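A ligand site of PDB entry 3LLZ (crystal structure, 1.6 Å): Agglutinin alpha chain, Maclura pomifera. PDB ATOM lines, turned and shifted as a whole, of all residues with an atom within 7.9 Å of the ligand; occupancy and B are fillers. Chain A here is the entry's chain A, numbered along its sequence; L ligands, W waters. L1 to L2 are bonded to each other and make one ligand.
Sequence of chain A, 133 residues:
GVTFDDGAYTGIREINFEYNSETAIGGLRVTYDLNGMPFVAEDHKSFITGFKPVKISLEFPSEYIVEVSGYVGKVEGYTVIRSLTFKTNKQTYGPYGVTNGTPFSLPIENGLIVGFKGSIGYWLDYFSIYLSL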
ATOM      1  N   GLY A   1      30.485  27.235 -29.193  1.00  0.00           N
ATOM      2  CA  GLY A   1      31.771  26.711 -28.647  1.00  0.00           C
ATOM      3  C   GLY A   1      32.328  25.596 -29.509  1.00  0.00           C
ATOM      4  O   GLY A   1      31.767  25.255 -30.548  1.00  0.00           O
ATOM      5  N   VAL A   2      33.458  25.027 -29.074  1.00  0.00           N
ATOM      6  CA  VAL A   2      34.064  23.928 -29.797  1.00  0.00           C
ATOM      7  C   VAL A   2      33.378  22.650 -29.332  1.00  0.00           C
ATOM      8  O   VAL A   2      33.360  22.354 -28.135  1.00  0.00           O
ATOM      9  CB  VAL A   2      35.579  23.837 -29.505  1.00  0.00           C
ATOM     10  CG1 VAL A   2      36.166  22.593 -30.171  1.00  0.00           C
ATOM     11  CG2 VAL A   2      36.283  25.094 -30.013  1.00  0.00           C
ATOM     12  N   THR A   3      32.813  21.899 -30.274  1.00  0.00           N
ATOM     13  CA  THR A   3      32.142  20.660 -29.914  1.00  0.00           C
ATOM     14  C   THR A   3      33.148  19.566 -29.621  1.00  0.00           C
ATOM     15  O   THR A   3      34.265  19.558 -30.141  1.00  0.00           O
ATOM     16  CB  THR A   3      31.221  20.164 -31.063  1.00  0.00           C
ATOM     17  OG1 THR A   3      32.003  19.968 -32.246  1.00  0.00           O
ATOM     18  CG2 THR A   3      30.126  21.183 -31.338  1.00  0.00           C
ATOM     19  N   ILE A  25      29.568  26.922 -15.679  1.00  0.00           N
ATOM     20  CA  ILE A  25      30.562  25.870 -15.766  1.00  0.00           C
ATOM     21  C   ILE A  25      31.523  26.193 -16.905  1.00  0.00           C
ATOM     22  O   ILE A  25      31.109  26.709 -17.943  1.00  0.00           O
ATOM     23  CB  ILE A  25      29.892  24.491 -16.051  1.00  0.00           C
ATOM     24  CG1 ILE A  25      28.906  24.149 -14.915  1.00  0.00           C
ATOM     25  CG2 ILE A  25      30.952  23.402 -16.184  1.00  0.00           C
ATOM     26  CD1 ILE A  25      29.536  24.095 -13.536  1.00  0.00           C
ATOM     27  N   SER A  46      37.842  25.903 -21.658  1.00  0.00           N
ATOM     28  CA  SER A  46      37.001  27.080 -21.785  1.00  0.00           C
ATOM     29  C   SER A  46      37.838  28.057 -22.600  1.00  0.00           C
ATOM     30  O   SER A  46      39.071  27.960 -22.621  1.00  0.00           O
ATOM     31  CB  SER A  46      36.712  27.676 -20.413  1.00  0.00           C
ATOM     32  OG  SER A  46      36.276  29.025 -20.539  1.00  0.00           O
ATOM     33  N   PHE A  47      37.181  29.004 -23.270  1.00  0.00           N
ATOM     34  CA  PHE A  47      37.880  30.009 -24.053  1.00  0.00           C
ATOM     35  C   PHE A  47      38.535  31.032 -23.133  1.00  0.00           C
ATOM     36  O   PHE A  47      39.359  31.832 -23.569  1.00  0.00           O
ATOM     37  CB  PHE A  47      36.911  30.753 -24.975  1.00  0.00           C
ATOM     38  CG  PHE A  47      36.423  29.956 -26.172  1.00  0.00           C
ATOM     39  CD1 PHE A  47      35.585  30.552 -27.094  1.00  0.00           C
ATOM     40  CD2 PHE A  47      36.792  28.630 -26.350  1.00  0.00           C
ATOM     41  CE1 PHE A  47      35.107  29.844 -28.195  1.00  0.00           C
ATOM     42  CE2 PHE A  47      36.323  27.901 -27.450  1.00  0.00           C
ATOM     43  CZ  PHE A  47      35.480  28.510 -28.377  1.00  0.00           C
ATOM     44  N   ILE A  48      38.159  31.005 -21.857  1.00  0.00           N
ATOM     45  CA  ILE A  48      38.696  31.946 -20.873  1.00  0.00           C
ATOM     46  C   ILE A  48      39.151  31.307 -19.564  1.00  0.00           C
ATOM     47  O   ILE A  48      39.045  30.094 -19.368  1.00  0.00           O
ATOM     48  CB  ILE A  48      37.651  33.031 -20.529  1.00  0.00           C
ATOM     49  CG1 ILE A  48      36.379  32.372 -20.004  1.00  0.00           C
ATOM     50  CG2 ILE A  48      37.348  33.866 -21.758  1.00  0.00           C
ATOM     51  CD1 ILE A  48      35.385  33.359 -19.413  1.00  0.00           C
ATOM     52  N   VAL A  75      24.157  33.501 -19.704  1.00  0.00           N
ATOM     53  CA  VAL A  75      25.314  34.250 -19.242  1.00  0.00           C
ATOM     54  C   VAL A  75      25.733  35.015 -20.489  1.00  0.00           C
ATOM     55  O   VAL A  75      26.052  34.409 -21.515  1.00  0.00           O
ATOM     56  CB  VAL A  75      26.452  33.322 -18.768  1.00  0.00           C
ATOM     57  CG1 VAL A  75      27.665  34.148 -18.383  1.00  0.00           C
ATOM     58  CG2 VAL A  75      25.982  32.494 -17.578  1.00  0.00           C
ATOM     59  N   GLU A  76      25.706  36.336 -20.409  1.00  0.00           N
ATOM     60  CA  GLU A  76      26.055  37.176 -21.543  1.00  0.00           C
ATOM     61  C   GLU A  76      25.204  36.802 -22.755  1.00  0.00           C
ATOM     62  O   GLU A  76      25.667  36.859 -23.892  1.00  0.00           O
ATOM     63  CB  GLU A  76      27.555  37.069 -21.846  1.00  0.00           C
ATOM     64  CG  GLU A  76      28.420  37.850 -20.875  1.00  0.00           C
ATOM     65  CD  GLU A  76      29.901  37.545 -21.001  1.00  0.00           C
ATOM     66  OE1 GLU A  76      30.396  37.347 -22.130  1.00  0.00           O
ATOM     67  OE2 GLU A  76      30.591  37.517 -19.955  1.00  0.00           O
ATOM     68  N   GLY A  77      23.954  36.414 -22.500  1.00  0.00           N
ATOM     69  CA  GLY A  77      23.047  36.054 -23.579  1.00  0.00           C
ATOM     70  C   GLY A  77      23.116  34.632 -24.090  1.00  0.00           C
ATOM     71  O   GLY A  77      22.231  34.196 -24.835  1.00  0.00           O
ATOM     72  N   TYR A  78      24.168  33.898 -23.715  1.00  0.00           N
ATOM     73  CA  TYR A  78      24.318  32.519 -24.147  1.00  0.00           C
ATOM     74  C   TYR A  78      23.695  31.548 -23.159  1.00  0.00           C
ATOM     75  O   TYR A  78      23.882  31.670 -21.959  1.00  0.00           O
ATOM     76  CB  TYR A  78      25.812  32.178 -24.310  1.00  0.00           C
ATOM     77  CG  TYR A  78      26.465  32.834 -25.504  1.00  0.00           C
ATOM     78  CD1 TYR A  78      27.240  33.987 -25.352  1.00  0.00           C
ATOM     79  CD2 TYR A  78      26.324  32.304 -26.786  1.00  0.00           C
ATOM     80  CE1 TYR A  78      27.851  34.588 -26.452  1.00  0.00           C
ATOM     81  CE2 TYR A  78      26.925  32.902 -27.886  1.00  0.00           C
ATOM     82  CZ  TYR A  78      27.688  34.032 -27.718  1.00  0.00           C
ATOM     83  OH  TYR A  78      28.299  34.606 -28.808  1.00  0.00           O
ATOM     84  N   THR A  79      22.943  30.572 -23.681  1.00  0.00           N
ATOM     85  CA  THR A  79      22.306  29.579 -22.817  1.00  0.00           C
ATOM     86  C   THR A  79      23.352  28.519 -22.517  1.00  0.00           C
ATOM     87  O   THR A  79      23.815  27.821 -23.416  1.00  0.00           O
ATOM     88  CB  THR A  79      21.099  28.924 -23.517  1.00  0.00           C
ATOM     89  OG1 THR A  79      20.148  29.928 -23.873  1.00  0.00           O
ATOM     90  CG2 THR A  79      20.437  27.914 -22.580  1.00  0.00           C
ATOM     91  N   VAL A  80      23.734  28.410 -21.249  1.00  0.00           N
ATOM     92  CA  VAL A  80      24.767  27.474 -20.848  1.00  0.00           C
ATOM     93  C   VAL A  80      24.440  26.722 -19.578  1.00  0.00           C
ATOM     94  O   VAL A  80      23.449  26.999 -18.903  1.00  0.00           O
ATOM     95  CB  VAL A  80      26.104  28.216 -20.643  1.00  0.00           C
ATOM     96  CG1 VAL A  80      26.552  28.873 -21.935  1.00  0.00           C
ATOM     97  CG2 VAL A  80      25.947  29.274 -19.541  1.00  0.00           C
ATOM     98  N   ILE A  81      25.285  25.742 -19.261  1.00  0.00           N
ATOM     99  CA  ILE A  81      25.117  24.964 -18.035  1.00  0.00           C
ATOM    100  C   ILE A  81      25.770  25.800 -16.946  1.00  0.00           C
ATOM    101  O   ILE A  81      26.989  25.998 -16.944  1.00  0.00           O
ATOM    102  CB  ILE A  81      25.809  23.580 -18.144  1.00  0.00           C
ATOM    103  CG1 ILE A  81      25.140  22.728 -19.236  1.00  0.00           C
ATOM    104  CG2 ILE A  81      25.703  22.840 -16.817  1.00  0.00           C
ATOM    105  CD1 ILE A  81      25.207  23.314 -20.614  1.00  0.00           C
ATOM    106  N   SER A 119      29.676  20.735 -25.943  1.00  0.00           N
ATOM    107  CA  SER A 119      30.295  21.903 -26.557  1.00  0.00           C
ATOM    108  C   SER A 119      30.713  22.878 -25.489  1.00  0.00           C
ATOM    109  O   SER A 119      29.983  23.097 -24.531  1.00  0.00           O
ATOM    110  CB  SER A 119      29.295  22.586 -27.498  1.00  0.00           C
ATOM    111  OG  SER A 119      29.777  23.840 -27.951  1.00  0.00           O
ATOM    112  N   ILE A 120      31.902  23.460 -25.631  1.00  0.00           N
ATOM    113  CA  ILE A 120      32.374  24.431 -24.669  1.00  0.00           C
ATOM    114  C   ILE A 120      33.002  25.628 -25.371  1.00  0.00           C
ATOM    115  O   ILE A 120      33.858  25.475 -26.237  1.00  0.00           O
ATOM    116  CB  ILE A 120      33.429  23.829 -23.708  1.00  0.00           C
ATOM    117  CG1 ILE A 120      32.855  22.574 -23.036  1.00  0.00           C
ATOM    118  CG2 ILE A 120      33.815  24.864 -22.645  1.00  0.00           C
ATOM    119  CD1 ILE A 120      33.796  21.938 -22.015  1.00  0.00           C
ATOM    120  N   GLY A 121      32.528  26.815 -25.013  1.00  0.00           N
ATOM    121  CA  GLY A 121      33.055  28.059 -25.563  1.00  0.00           C
ATOM    122  C   GLY A 121      33.583  28.750 -24.325  1.00  0.00           C
ATOM    123  O   GLY A 121      34.480  28.242 -23.670  1.00  0.00           O
ATOM    124  N   TYR A 122      33.033  29.911 -23.997  1.00  0.00           N
ATOM    125  CA  TYR A 122      33.451  30.583 -22.781  1.00  0.00           C
ATOM    126  C   TYR A 122      32.986  29.681 -21.630  1.00  0.00           C
ATOM    127  O   TYR A 122      33.667  29.561 -20.617  1.00  0.00           O
ATOM    128  CB  TYR A 122      32.784  31.957 -22.680  1.00  0.00           C
ATOM    129  CG  TYR A 122      33.549  33.044 -23.410  1.00  0.00           C
ATOM    130  CD1 TYR A 122      33.844  32.913 -24.764  1.00  0.00           C
ATOM    131  CD2 TYR A 122      33.998  34.177 -22.741  1.00  0.00           C
ATOM    132  CE1 TYR A 122      34.579  33.884 -25.436  1.00  0.00           C
ATOM    133  CE2 TYR A 122      34.740  35.157 -23.400  1.00  0.00           C
ATOM    134  CZ  TYR A 122      35.024  34.998 -24.751  1.00  0.00           C
ATOM    135  OH  TYR A 122      35.773  35.962 -25.395  1.00  0.00           O
ATOM    136  N   TRP A 123      31.844  29.044 -21.828  1.00  0.00           N
ATOM    137  CA  TRP A 123      31.271  28.141 -20.823  1.00  0.00           C
ATOM    138  C   TRP A 123      30.754  26.877 -21.487  1.00  0.00           C
ATOM    139  O   TRP A 123      30.701  26.769 -22.713  1.00  0.00           O
ATOM    140  CB  TRP A 123      30.127  28.853 -20.093  1.00  0.00           C
ATOM    141  CG  TRP A 123      30.567  30.148 -19.514  1.00  0.00           C
ATOM    142  CD1 TRP A 123      31.390  30.335 -18.453  1.00  0.00           C
ATOM    143  CD2 TRP A 123      30.311  31.455 -20.060  1.00  0.00           C
ATOM    144  NE1 TRP A 123      31.682  31.664 -18.300  1.00  0.00           N
ATOM    145  CE2 TRP A 123      31.034  32.377 -19.274  1.00  0.00           C
ATOM    146  CE3 TRP A 123      29.549  31.928 -21.136  1.00  0.00           C
ATOM    147  CZ2 TRP A 123      31.023  33.755 -19.530  1.00  0.00           C
ATOM    148  CZ3 TRP A 123      29.541  33.298 -21.396  1.00  0.00           C
ATOM    149  CH2 TRP A 123      30.275  34.192 -20.589  1.00  0.00           C
ATOM    150  N   LEU A 124      30.373  25.911 -20.652  1.00  0.00           N
ATOM    151  CA  LEU A 124      29.814  24.651 -21.147  1.00  0.00           C
ATOM    152  C   LEU A 124      28.462  24.979 -21.776  1.00  0.00           C
ATOM    153  O   LEU A 124      27.513  25.313 -21.065  1.00  0.00           O
ATOM    154  CB  LEU A 124      29.653  23.683 -19.981  1.00  0.00           C
ATOM    155  CG  LEU A 124      29.005  22.327 -20.271  1.00  0.00           C
ATOM    156  CD1 LEU A 124      29.795  21.579 -21.335  1.00  0.00           C
ATOM    157  CD2 LEU A 124      28.935  21.521 -18.974  1.00  0.00           C
ATOM    158  N   ASP A 125      28.384  24.902 -23.094  1.00  0.00           N
ATOM    159  CA  ASP A 125      27.149  25.228 -23.806  1.00  0.00           C
ATOM    160  C   ASP A 125      26.053  24.206 -23.571  1.00  0.00           C
ATOM    161  O   ASP A 125      24.887  24.558 -23.337  1.00  0.00           O
ATOM    162  CB  ASP A 125      27.419  25.329 -25.296  1.00  0.00           C
ATOM    163  CG  ASP A 125      28.501  26.328 -25.624  1.00  0.00           C
ATOM    164  OD1 ASP A 125      28.360  27.510 -25.233  1.00  0.00           O
ATOM    165  OD2 ASP A 125      29.486  25.927 -26.279  1.00  0.00           O
ATOM    166  N   TYR A 126      26.420  22.945 -23.660  1.00  0.00           N
ATOM    167  CA  TYR A 126      25.477  21.855 -23.484  1.00  0.00           C
ATOM    168  C   TYR A 126      26.282  20.571 -23.434  1.00  0.00           C
ATOM    169  O   TYR A 126      27.470  20.556 -23.741  1.00  0.00           O
ATOM    170  CB  TYR A 126      24.488  21.791 -24.657  1.00  0.00           C
ATOM    171  CG  TYR A 126      25.127  21.682 -26.034  1.00  0.00           C
ATOM    172  CD1 TYR A 126      25.245  22.809 -26.855  1.00  0.00           C
ATOM    173  CD2 TYR A 126      25.600  20.465 -26.511  1.00  0.00           C
ATOM    174  CE1 TYR A 126      25.827  22.713 -28.121  1.00  0.00           C
ATOM    175  CE2 TYR A 126      26.177  20.356 -27.781  1.00  0.00           C
ATOM    176  CZ  TYR A 126      26.291  21.494 -28.576  1.00  0.00           C
ATOM    177  OH  TYR A 126      26.867  21.387 -29.823  1.00  0.00           O
HETATM  178  C1  LIG L   1      31.571  31.627 -27.479  1.00  0.00           C
HETATM  179  C2  LIG L   1      31.181  30.657 -28.615  1.00  0.00           C
HETATM  180  C3  LIG L   1      29.662  30.546 -28.625  1.00  0.00           C
HETATM  181  C4  LIG L   1      29.196  29.999 -27.258  1.00  0.00           C
HETATM  182  C5  LIG L   1      29.659  30.998 -26.177  1.00  0.00           C
HETATM  183  C6  LIG L   1      29.261  30.612 -24.750  1.00  0.00           C
HETATM  184  C7  LIG L   1      32.315  30.338 -30.715  1.00  0.00           C
HETATM  185  C8  LIG L   1      32.868  30.945 -31.987  1.00  0.00           C
HETATM  186  N1  LIG L   1      31.658  31.154 -29.883  1.00  0.00           N
HETATM  187  O1  LIG L   1      32.953  31.734 -27.416  1.00  0.00           O
HETATM  188  O2  LIG L   1      29.172  29.732 -29.731  1.00  0.00           O
HETATM  189  O3  LIG L   1      29.775  28.728 -27.028  1.00  0.00           O
HETATM  190  O4  LIG L   1      31.096  31.155 -26.212  1.00  0.00           O
HETATM  191  O5  LIG L   1      30.032  29.524 -24.246  1.00  0.00           O
HETATM  192  O6  LIG L   1      32.482  29.141 -30.481  1.00  0.00           O
HETATM  193  C1  LG2 L   2      28.217  30.446 -30.462  1.00  0.00           C
HETATM  194  C2  LG2 L   2      28.477  29.317 -31.498  1.00  0.00           C
HETATM  195  C3  LG2 L   2      27.359  29.289 -32.542  1.00  0.00           C
HETATM  196  C4  LG2 L   2      25.956  29.324 -31.903  1.00  0.00           C
HETATM  197  C5  LG2 L   2      25.872  30.386 -30.800  1.00  0.00           C
HETATM  198  C6  LG2 L   2      24.574  30.317 -30.012  1.00  0.00           C
HETATM  199  O1  LG2 L   2      29.723  29.528 -32.151  1.00  0.00           O
HETATM  200  O2  LG2 L   2      27.469  28.142 -33.367  1.00  0.00           O
HETATM  201  O3  LG2 L   2      25.634  28.046 -31.364  1.00  0.00           O
HETATM  202  O4  LG2 L   2      26.947  30.212 -29.857  1.00  0.00           O
HETATM  203  O5  LG2 L   2      23.569  31.113 -30.630  1.00  0.00           O
HETATM  204  O   HOH W   1      26.846  25.768 -34.078  1.00  0.00           O
HETATM  205  O   HOH W   2      26.266  26.691 -29.161  1.00  0.00           O
HETATM  206  O   HOH W   3      30.693  26.928 -32.858  1.00  0.00           O
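Water W3 lies within hydrogen-bond range of an oxygen (O1) of LG2 L2 (2.9 Å) and the backbone carbonyl oxygen of Gly 1 (3.0 Å).
Residues that only touch the ligand: Phe 47, Tyr 78 and Gly 121. Hydrophobic or aromatic side chains within 4 Å of the ligand: Phe 47, Tyr 78, Tyr 122 and Trp 123. Within 4 Å of the ligand: Gly 1, Phe 47, Tyr 78, Gly 121, Tyr 122, Trp 123 and Asp 125. The nearest printed residue that does not touch the ligand is Val 80 (4.2 Å).
An oxygen (O3) of LIG L1 is in hydrogen-bond range of the side-chain carboxylate of Asp 125, at 2.6 Å. The backbone NH (N) of Gly 1 is in hydrogen-bond range of an oxygen (O3) of LIG L1 (2.7 Å). The backbone NH (N) of Trp 123 is in hydrogen-bond range of an oxygen (O5) of LIG L1 (3.1 Å). The backbone NH (N) of Tyr 122 is in hydrogen-bond range of an oxygen (O5) of LIG L1, 3.0 Å away. An oxygen (O5) of LIG L1 lies within hydrogen-bond range of the backbone carbonyl oxygen of Trp 123 (3.2 Å).
OD2 of Asp 125 sits at hydrogen-bond distance from N of Gly 1, 3.3 Å away. The backbone NH (N) of Gly 121 is in hydrogen-bond range of the side-chain carboxylate (OD2) of Asp 125, at 3.4 Å. The backbone carbonyl oxygen (O) of Gly 121 lies within hydrogen-bond range of the backbone NH (N) of Phe 47. O of Tyr 122 is in hydrogen-bond range of OG of Ser 46 (2.7 Å). The side-chain hydroxyl of Ser 119 sits at hydrogen-bond distance from the side-chain carboxylate of Asp 125, at 2.7 Å.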
